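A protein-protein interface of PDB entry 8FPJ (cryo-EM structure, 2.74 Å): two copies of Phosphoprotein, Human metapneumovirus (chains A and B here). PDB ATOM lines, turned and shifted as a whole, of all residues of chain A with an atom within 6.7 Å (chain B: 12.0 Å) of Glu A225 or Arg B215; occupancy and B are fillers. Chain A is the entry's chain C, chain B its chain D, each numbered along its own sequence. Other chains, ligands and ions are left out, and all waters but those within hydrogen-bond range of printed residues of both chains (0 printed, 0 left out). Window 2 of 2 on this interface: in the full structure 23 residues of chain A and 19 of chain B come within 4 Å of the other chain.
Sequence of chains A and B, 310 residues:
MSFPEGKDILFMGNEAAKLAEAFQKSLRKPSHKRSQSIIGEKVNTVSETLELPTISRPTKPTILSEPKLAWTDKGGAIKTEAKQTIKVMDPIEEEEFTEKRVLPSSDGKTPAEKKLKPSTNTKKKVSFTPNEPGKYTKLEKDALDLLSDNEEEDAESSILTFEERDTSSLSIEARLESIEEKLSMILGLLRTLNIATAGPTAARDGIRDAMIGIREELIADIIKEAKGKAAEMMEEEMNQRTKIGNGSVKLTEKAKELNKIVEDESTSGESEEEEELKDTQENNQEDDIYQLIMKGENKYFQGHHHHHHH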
ATOM      1  N   GLU A 217       7.702  -6.121   0.568  1.00  0.00           N
ATOM      2  CA  GLU A 217       8.029  -5.188  -0.500  1.00  0.00           C
ATOM      3  C   GLU A 217       9.179  -5.681  -1.360  1.00  0.00           C
ATOM      4  O   GLU A 217       9.138  -5.539  -2.581  1.00  0.00           O
ATOM      5  CB  GLU A 217       8.381  -3.818   0.092  1.00  0.00           C
ATOM      6  CG  GLU A 217       8.690  -2.748  -0.930  1.00  0.00           C
ATOM      7  CD  GLU A 217       7.486  -2.407  -1.775  1.00  0.00           C
ATOM      8  OE1 GLU A 217       6.353  -2.602  -1.291  1.00  0.00           O
ATOM      9  OE2 GLU A 217       7.668  -1.950  -2.922  1.00  0.00           O
ATOM     10  N   LEU A 218      10.211  -6.250  -0.734  1.00  0.00           N
ATOM     11  CA  LEU A 218      11.209  -7.001  -1.482  1.00  0.00           C
ATOM     12  C   LEU A 218      10.621  -8.295  -2.030  1.00  0.00           C
ATOM     13  O   LEU A 218      11.136  -8.845  -3.009  1.00  0.00           O
ATOM     14  CB  LEU A 218      12.409  -7.296  -0.583  1.00  0.00           C
ATOM     15  CG  LEU A 218      13.696  -7.746  -1.272  1.00  0.00           C
ATOM     16  CD1 LEU A 218      14.335  -6.598  -2.030  1.00  0.00           C
ATOM     17  CD2 LEU A 218      14.660  -8.310  -0.245  1.00  0.00           C
ATOM     18  N   ILE A 219       9.549  -8.793  -1.413  1.00  0.00           N
ATOM     19  CA  ILE A 219       8.914 -10.020  -1.885  1.00  0.00           C
ATOM     20  C   ILE A 219       8.227  -9.784  -3.224  1.00  0.00           C
ATOM     21  O   ILE A 219       8.311 -10.610  -4.140  1.00  0.00           O
ATOM     22  CB  ILE A 219       7.926 -10.547  -0.830  1.00  0.00           C
ATOM     23  CG1 ILE A 219       8.695 -11.154   0.343  1.00  0.00           C
ATOM     24  CG2 ILE A 219       6.981 -11.559  -1.452  1.00  0.00           C
ATOM     25  CD1 ILE A 219       7.863 -11.354   1.582  1.00  0.00           C
ATOM     26  N   ALA A 220       7.517  -8.663  -3.352  1.00  0.00           N
ATOM     27  CA  ALA A 220       6.880  -8.344  -4.623  1.00  0.00           C
ATOM     28  C   ALA A 220       7.920  -8.112  -5.710  1.00  0.00           C
ATOM     29  O   ALA A 220       7.718  -8.495  -6.868  1.00  0.00           O
ATOM     30  CB  ALA A 220       5.981  -7.119  -4.467  1.00  0.00           C
ATOM     31  N   ASP A 221       9.041  -7.484  -5.355  1.00  0.00           N
ATOM     32  CA  ASP A 221      10.078  -7.192  -6.339  1.00  0.00           C
ATOM     33  C   ASP A 221      10.642  -8.472  -6.947  1.00  0.00           C
ATOM     34  O   ASP A 221      10.816  -8.569  -8.167  1.00  0.00           O
ATOM     35  CB  ASP A 221      11.190  -6.371  -5.689  1.00  0.00           C
ATOM     36  CG  ASP A 221      12.234  -5.913  -6.683  1.00  0.00           C
ATOM     37  OD1 ASP A 221      11.945  -4.987  -7.468  1.00  0.00           O
ATOM     38  OD2 ASP A 221      13.345  -6.481  -6.679  1.00  0.00           O
ATOM     39  N   ILE A 222      10.938  -9.468  -6.109  1.00  0.00           N
ATOM     40  CA  ILE A 222      11.532 -10.702  -6.616  1.00  0.00           C
ATOM     41  C   ILE A 222      10.530 -11.467  -7.472  1.00  0.00           C
ATOM     42  O   ILE A 222      10.901 -12.093  -8.472  1.00  0.00           O
ATOM     43  CB  ILE A 222      12.066 -11.567  -5.458  1.00  0.00           C
ATOM     44  CG1 ILE A 222      10.951 -11.911  -4.469  1.00  0.00           C
ATOM     45  CG2 ILE A 222      13.205 -10.851  -4.751  1.00  0.00           C
ATOM     46  CD1 ILE A 222      11.413 -12.742  -3.293  1.00  0.00           C
ATOM     47  N   ILE A 223       9.250 -11.440  -7.096  1.00  0.00           N
ATOM     48  CA  ILE A 223       8.237 -12.137  -7.882  1.00  0.00           C
ATOM     49  C   ILE A 223       8.135 -11.535  -9.279  1.00  0.00           C
ATOM     50  O   ILE A 223       8.047 -12.258 -10.277  1.00  0.00           O
ATOM     51  CB  ILE A 223       6.880 -12.106  -7.153  1.00  0.00           C
ATOM     52  CG1 ILE A 223       6.968 -12.880  -5.836  1.00  0.00           C
ATOM     53  CG2 ILE A 223       5.787 -12.686  -8.042  1.00  0.00           C
ATOM     54  CD1 ILE A 223       5.779 -12.676  -4.922  1.00  0.00           C
ATOM     55  N   LYS A 224       8.145 -10.204  -9.372  1.00  0.00           N
ATOM     56  CA  LYS A 224       7.971  -9.553 -10.668  1.00  0.00           C
ATOM     57  C   LYS A 224       9.093  -9.930 -11.628  1.00  0.00           C
ATOM     58  O   LYS A 224       8.844 -10.244 -12.797  1.00  0.00           O
ATOM     59  CB  LYS A 224       7.900  -8.037 -10.488  1.00  0.00           C
ATOM     60  CG  LYS A 224       6.496  -7.470 -10.628  1.00  0.00           C
ATOM     61  CD  LYS A 224       6.431  -6.015 -10.192  1.00  0.00           C
ATOM     62  CE  LYS A 224       7.221  -5.113 -11.123  1.00  0.00           C
ATOM     63  NZ  LYS A 224       7.033  -3.675 -10.789  1.00  0.00           N
ATOM     64  N   GLU A 225      10.341  -9.904 -11.156  1.00  0.00           N
ATOM     65  CA  GLU A 225      11.450 -10.292 -12.022  1.00  0.00           C
ATOM     66  C   GLU A 225      11.417 -11.786 -12.315  1.00  0.00           C
ATOM     67  O   GLU A 225      11.762 -12.215 -13.422  1.00  0.00           O
ATOM     68  CB  GLU A 225      12.786  -9.898 -11.392  1.00  0.00           C
ATOM     69  CG  GLU A 225      13.123 -10.630 -10.105  1.00  0.00           C
ATOM     70  CD  GLU A 225      14.426 -10.153  -9.493  1.00  0.00           C
ATOM     71  OE1 GLU A 225      15.053  -9.237 -10.066  1.00  0.00           O
ATOM     72  OE2 GLU A 225      14.827 -10.694  -8.440  1.00  0.00           O
ATOM     73  N   ALA A 226      11.006 -12.595 -11.336  1.00  0.00           N
ATOM     74  CA  ALA A 226      10.888 -14.031 -11.572  1.00  0.00           C
ATOM     75  C   ALA A 226       9.831 -14.326 -12.626  1.00  0.00           C
ATOM     76  O   ALA A 226      10.055 -15.139 -13.531  1.00  0.00           O
ATOM     77  CB  ALA A 226      10.558 -14.751 -10.266  1.00  0.00           C
ATOM     78  N   LYS A 227       8.671 -13.675 -12.529  1.00  0.00           N
ATOM     79  CA  LYS A 227       7.633 -13.868 -13.534  1.00  0.00           C
ATOM     80  C   LYS A 227       7.996 -13.193 -14.851  1.00  0.00           C
ATOM     81  O   LYS A 227       7.672 -13.716 -15.923  1.00  0.00           O
ATOM     82  CB  LYS A 227       6.295 -13.339 -13.018  1.00  0.00           C
ATOM     83  CG  LYS A 227       5.665 -14.214 -11.947  1.00  0.00           C
ATOM     84  CD  LYS A 227       4.279 -13.721 -11.569  1.00  0.00           C
ATOM     85  CE  LYS A 227       3.579 -14.701 -10.642  1.00  0.00           C
ATOM     86  NZ  LYS A 227       2.231 -14.222 -10.236  1.00  0.00           N
ATOM     87  N   GLY A 228       8.661 -12.038 -14.795  1.00  0.00           N
ATOM     88  CA  GLY A 228       9.081 -11.384 -16.023  1.00  0.00           C
ATOM     89  C   GLY A 228      10.038 -12.240 -16.828  1.00  0.00           C
ATOM     90  O   GLY A 228       9.918 -12.352 -18.050  1.00  0.00           O
ATOM     91  N   LYS A 229      11.011 -12.855 -16.149  1.00  0.00           N
ATOM     92  CA  LYS A 229      11.913 -13.776 -16.830  1.00  0.00           C
ATOM     93  C   LYS A 229      11.163 -15.004 -17.332  1.00  0.00           C
ATOM     94  O   LYS A 229      11.417 -15.486 -18.442  1.00  0.00           O
ATOM     95  CB  LYS A 229      13.051 -14.182 -15.893  1.00  0.00           C
ATOM     96  CG  LYS A 229      14.088 -13.089 -15.682  1.00  0.00           C
ATOM     97  CD  LYS A 229      15.339 -13.619 -14.999  1.00  0.00           C
ATOM     98  CE  LYS A 229      15.081 -13.933 -13.534  1.00  0.00           C
ATOM     99  NZ  LYS A 229      16.332 -14.281 -12.805  1.00  0.00           N
ATOM    100  N   ALA A 230      10.235 -15.527 -16.526  1.00  0.00           N
ATOM    101  CA  ALA A 230       9.439 -16.670 -16.962  1.00  0.00           C
ATOM    102  C   ALA A 230       8.587 -16.316 -18.173  1.00  0.00           C
ATOM    103  O   ALA A 230       8.458 -17.118 -19.105  1.00  0.00           O
ATOM    104  CB  ALA A 230       8.561 -17.165 -15.813  1.00  0.00           C
ATOM    105  N   ILE B 207      26.195 -14.935   6.557  1.00  0.00           N
ATOM    106  CA  ILE B 207      24.824 -14.850   6.068  1.00  0.00           C
ATOM    107  C   ILE B 207      24.721 -14.028   4.789  1.00  0.00           C
ATOM    108  O   ILE B 207      23.721 -14.136   4.068  1.00  0.00           O
ATOM    109  CB  ILE B 207      23.901 -14.268   7.156  1.00  0.00           C
ATOM    110  CG1 ILE B 207      23.982 -15.103   8.437  1.00  0.00           C
ATOM    111  CG2 ILE B 207      22.466 -14.201   6.656  1.00  0.00           C
ATOM    112  CD1 ILE B 207      23.353 -14.435   9.642  1.00  0.00           C
ATOM    113  N   ARG B 208      25.731 -13.211   4.480  1.00  0.00           N
ATOM    114  CA  ARG B 208      25.645 -12.358   3.299  1.00  0.00           C
ATOM    115  C   ARG B 208      25.543 -13.182   2.023  1.00  0.00           C
ATOM    116  O   ARG B 208      24.816 -12.803   1.098  1.00  0.00           O
ATOM    117  CB  ARG B 208      26.856 -11.426   3.232  1.00  0.00           C
ATOM    118  CG  ARG B 208      26.750 -10.347   2.161  1.00  0.00           C
ATOM    119  CD  ARG B 208      28.112  -9.788   1.789  1.00  0.00           C
ATOM    120  NE  ARG B 208      28.048  -8.366   1.471  1.00  0.00           N
ATOM    121  CZ  ARG B 208      27.920  -7.866   0.249  1.00  0.00           C
ATOM    122  NH1 ARG B 208      27.839  -8.647  -0.817  1.00  0.00           N
ATOM    123  NH2 ARG B 208      27.872  -6.546   0.091  1.00  0.00           N
ATOM    124  N   ASP B 209      26.269 -14.299   1.945  1.00  0.00           N
ATOM    125  CA  ASP B 209      26.195 -15.140   0.756  1.00  0.00           C
ATOM    126  C   ASP B 209      24.780 -15.661   0.542  1.00  0.00           C
ATOM    127  O   ASP B 209      24.245 -15.597  -0.571  1.00  0.00           O
ATOM    128  CB  ASP B 209      27.181 -16.301   0.876  1.00  0.00           C
ATOM    129  CG  ASP B 209      28.608 -15.884   0.587  1.00  0.00           C
ATOM    130  OD1 ASP B 209      28.866 -15.365  -0.520  1.00  0.00           O
ATOM    131  OD2 ASP B 209      29.474 -16.077   1.466  1.00  0.00           O
ATOM    132  N   ALA B 210      24.150 -16.168   1.605  1.00  0.00           N
ATOM    133  CA  ALA B 210      22.779 -16.647   1.482  1.00  0.00           C
ATOM    134  C   ALA B 210      21.836 -15.516   1.096  1.00  0.00           C
ATOM    135  O   ALA B 210      20.978 -15.688   0.223  1.00  0.00           O
ATOM    136  CB  ALA B 210      22.328 -17.295   2.789  1.00  0.00           C
ATOM    137  N   MET B 211      21.989 -14.345   1.721  1.00  0.00           N
ATOM    138  CA  MET B 211      21.108 -13.228   1.396  1.00  0.00           C
ATOM    139  C   MET B 211      21.228 -12.846  -0.073  1.00  0.00           C
ATOM    140  O   MET B 211      20.217 -12.621  -0.749  1.00  0.00           O
ATOM    141  CB  MET B 211      21.423 -12.031   2.293  1.00  0.00           C
ATOM    142  CG  MET B 211      21.122 -12.267   3.760  1.00  0.00           C
ATOM    143  SD  MET B 211      19.379 -12.618   4.058  1.00  0.00           S
ATOM    144  CE  MET B 211      18.661 -11.020   3.697  1.00  0.00           C
ATOM    145  N   ILE B 212      22.456 -12.772  -0.588  1.00  0.00           N
ATOM    146  CA  ILE B 212      22.643 -12.545  -2.016  1.00  0.00           C
ATOM    147  C   ILE B 212      22.089 -13.701  -2.840  1.00  0.00           C
ATOM    148  O   ILE B 212      21.777 -13.515  -4.023  1.00  0.00           O
ATOM    149  CB  ILE B 212      24.129 -12.325  -2.348  1.00  0.00           C
ATOM    150  CG1 ILE B 212      24.675 -11.103  -1.601  1.00  0.00           C
ATOM    151  CG2 ILE B 212      24.325 -12.162  -3.851  1.00  0.00           C
ATOM    152  CD1 ILE B 212      24.109  -9.774  -2.075  1.00  0.00           C
ATOM    153  N   GLY B 213      21.956 -14.886  -2.249  1.00  0.00           N
ATOM    154  CA  GLY B 213      21.411 -16.027  -2.959  1.00  0.00           C
ATOM    155  C   GLY B 213      19.897 -16.116  -2.940  1.00  0.00           C
ATOM    156  O   GLY B 213      19.309 -16.796  -3.785  1.00  0.00           O
ATOM    157  N   ILE B 214      19.247 -15.441  -1.986  1.00  0.00           N
ATOM    158  CA  ILE B 214      17.790 -15.522  -1.888  1.00  0.00           C
ATOM    159  C   ILE B 214      17.126 -14.918  -3.117  1.00  0.00           C
ATOM    160  O   ILE B 214      16.100 -15.424  -3.588  1.00  0.00           O
ATOM    161  CB  ILE B 214      17.293 -14.845  -0.596  1.00  0.00           C
ATOM    162  CG1 ILE B 214      17.752 -15.637   0.631  1.00  0.00           C
ATOM    163  CG2 ILE B 214      15.774 -14.717  -0.615  1.00  0.00           C
ATOM    164  CD1 ILE B 214      17.548 -14.915   1.948  1.00  0.00           C
ATOM    165  N   ARG B 215      17.685 -13.830  -3.652  1.00  0.00           N
ATOM    166  CA  ARG B 215      17.092 -13.207  -4.831  1.00  0.00           C
ATOM    167  C   ARG B 215      17.007 -14.182  -5.998  1.00  0.00           C
ATOM    168  O   ARG B 215      16.138 -14.037  -6.865  1.00  0.00           O
ATOM    169  CB  ARG B 215      17.900 -11.974  -5.236  1.00  0.00           C
ATOM    170  CG  ARG B 215      17.921 -10.865  -4.193  1.00  0.00           C
ATOM    171  CD  ARG B 215      16.705  -9.960  -4.314  1.00  0.00           C
ATOM    172  NE  ARG B 215      16.727  -9.177  -5.545  1.00  0.00           N
ATOM    173  CZ  ARG B 215      15.759  -8.358  -5.934  1.00  0.00           C
ATOM    174  NH1 ARG B 215      14.674  -8.169  -5.200  1.00  0.00           N
ATOM    175  NH2 ARG B 215      15.883  -7.711  -7.089  1.00  0.00           N
ATOM    176  N   GLU B 216      17.894 -15.176  -6.039  1.00  0.00           N
ATOM    177  CA  GLU B 216      17.926 -16.157  -7.114  1.00  0.00           C
ATOM    178  C   GLU B 216      17.471 -17.543  -6.675  1.00  0.00           C
ATOM    179  O   GLU B 216      17.404 -18.449  -7.511  1.00  0.00           O
ATOM    180  CB  GLU B 216      19.340 -16.245  -7.699  1.00  0.00           C
ATOM    181  CG  GLU B 216      19.744 -15.028  -8.517  1.00  0.00           C
ATOM    182  CD  GLU B 216      21.184 -15.091  -8.986  1.00  0.00           C
ATOM    183  OE1 GLU B 216      22.032 -15.624  -8.240  1.00  0.00           O
ATOM    184  OE2 GLU B 216      21.468 -14.607 -10.101  1.00  0.00           O
ATOM    185  N   GLU B 217      17.159 -17.734  -5.394  1.00  0.00           N
ATOM    186  CA  GLU B 217      16.702 -19.026  -4.898  1.00  0.00           C
ATOM    187  C   GLU B 217      15.198 -19.224  -5.040  1.00  0.00           C
ATOM    188  O   GLU B 217      14.710 -20.328  -4.774  1.00  0.00           O
ATOM    189  CB  GLU B 217      17.086 -19.194  -3.424  1.00  0.00           C
ATOM    190  CG  GLU B 217      18.498 -19.707  -3.198  1.00  0.00           C
ATOM    191  CD  GLU B 217      18.968 -19.506  -1.769  1.00  0.00           C
ATOM    192  OE1 GLU B 217      19.084 -18.340  -1.337  1.00  0.00           O
ATOM    193  OE2 GLU B 217      19.217 -20.514  -1.074  1.00  0.00           O
ATOM    194  N   LEU B 218      14.461 -18.196  -5.447  1.00  0.00           N
ATOM    195  CA  LEU B 218      13.005 -18.272  -5.516  1.00  0.00           C
ATOM    196  C   LEU B 218      12.526 -18.262  -6.964  1.00  0.00           C
ATOM    197  O   LEU B 218      11.893 -17.308  -7.416  1.00  0.00           O
ATOM    198  CB  LEU B 218      12.381 -17.110  -4.742  1.00  0.00           C
ATOM    199  CG  LEU B 218      12.238 -17.310  -3.231  1.00  0.00           C
ATOM    200  CD1 LEU B 218      13.556 -17.716  -2.598  1.00  0.00           C
ATOM    201  CD2 LEU B 218      11.721 -16.043  -2.589  1.00  0.00           C
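The side-chain carboxylate (OD2) of Asp A221 lies within salt-bridge range of the guanidinium group (NH1) of Arg B215 (2.6 Å). The side-chain carboxylate (OE2) of Glu A225 lies within salt-bridge range of the guanidinium group (NH2) of Arg B215 (3.4 Å).
Arg B215 touches Leu A218. Ile A222 touches Arg B215. Ile A222 touches Leu B218.
Glu A225 touches just one residue of chain B: Arg B215. Of chain A, only Leu A218, Asp A221, Ile A222 and Glu A225 come within 4 Å of Arg B215. Leu A218 touches just one residue of chain B: Arg B215. Ile A222 touches just these residues of chain B: Arg B215 and Leu B218. Lys A224 touches none of the printed residues of chain B. No residue of chain B comes within 4 Å of Gly A228. No residue of chain B comes within 4 Å of Lys A229. Of the printed residues of chain A, Leu B218 touches Ile A222 (3.4 Å).
Hydrophobic or aromatic side chains of chain A within 4 Å of the printed part of chain B: Leu A218 and Ile A222. Hydrophobic or aromatic side chains of chain B within 4 Å of the printed part of chain A: Leu B218.
2 positions are printed for both chains. Of the 5 pairs that touch across the chains among the printed residues, none has its exchanged pair printed and touching as well.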
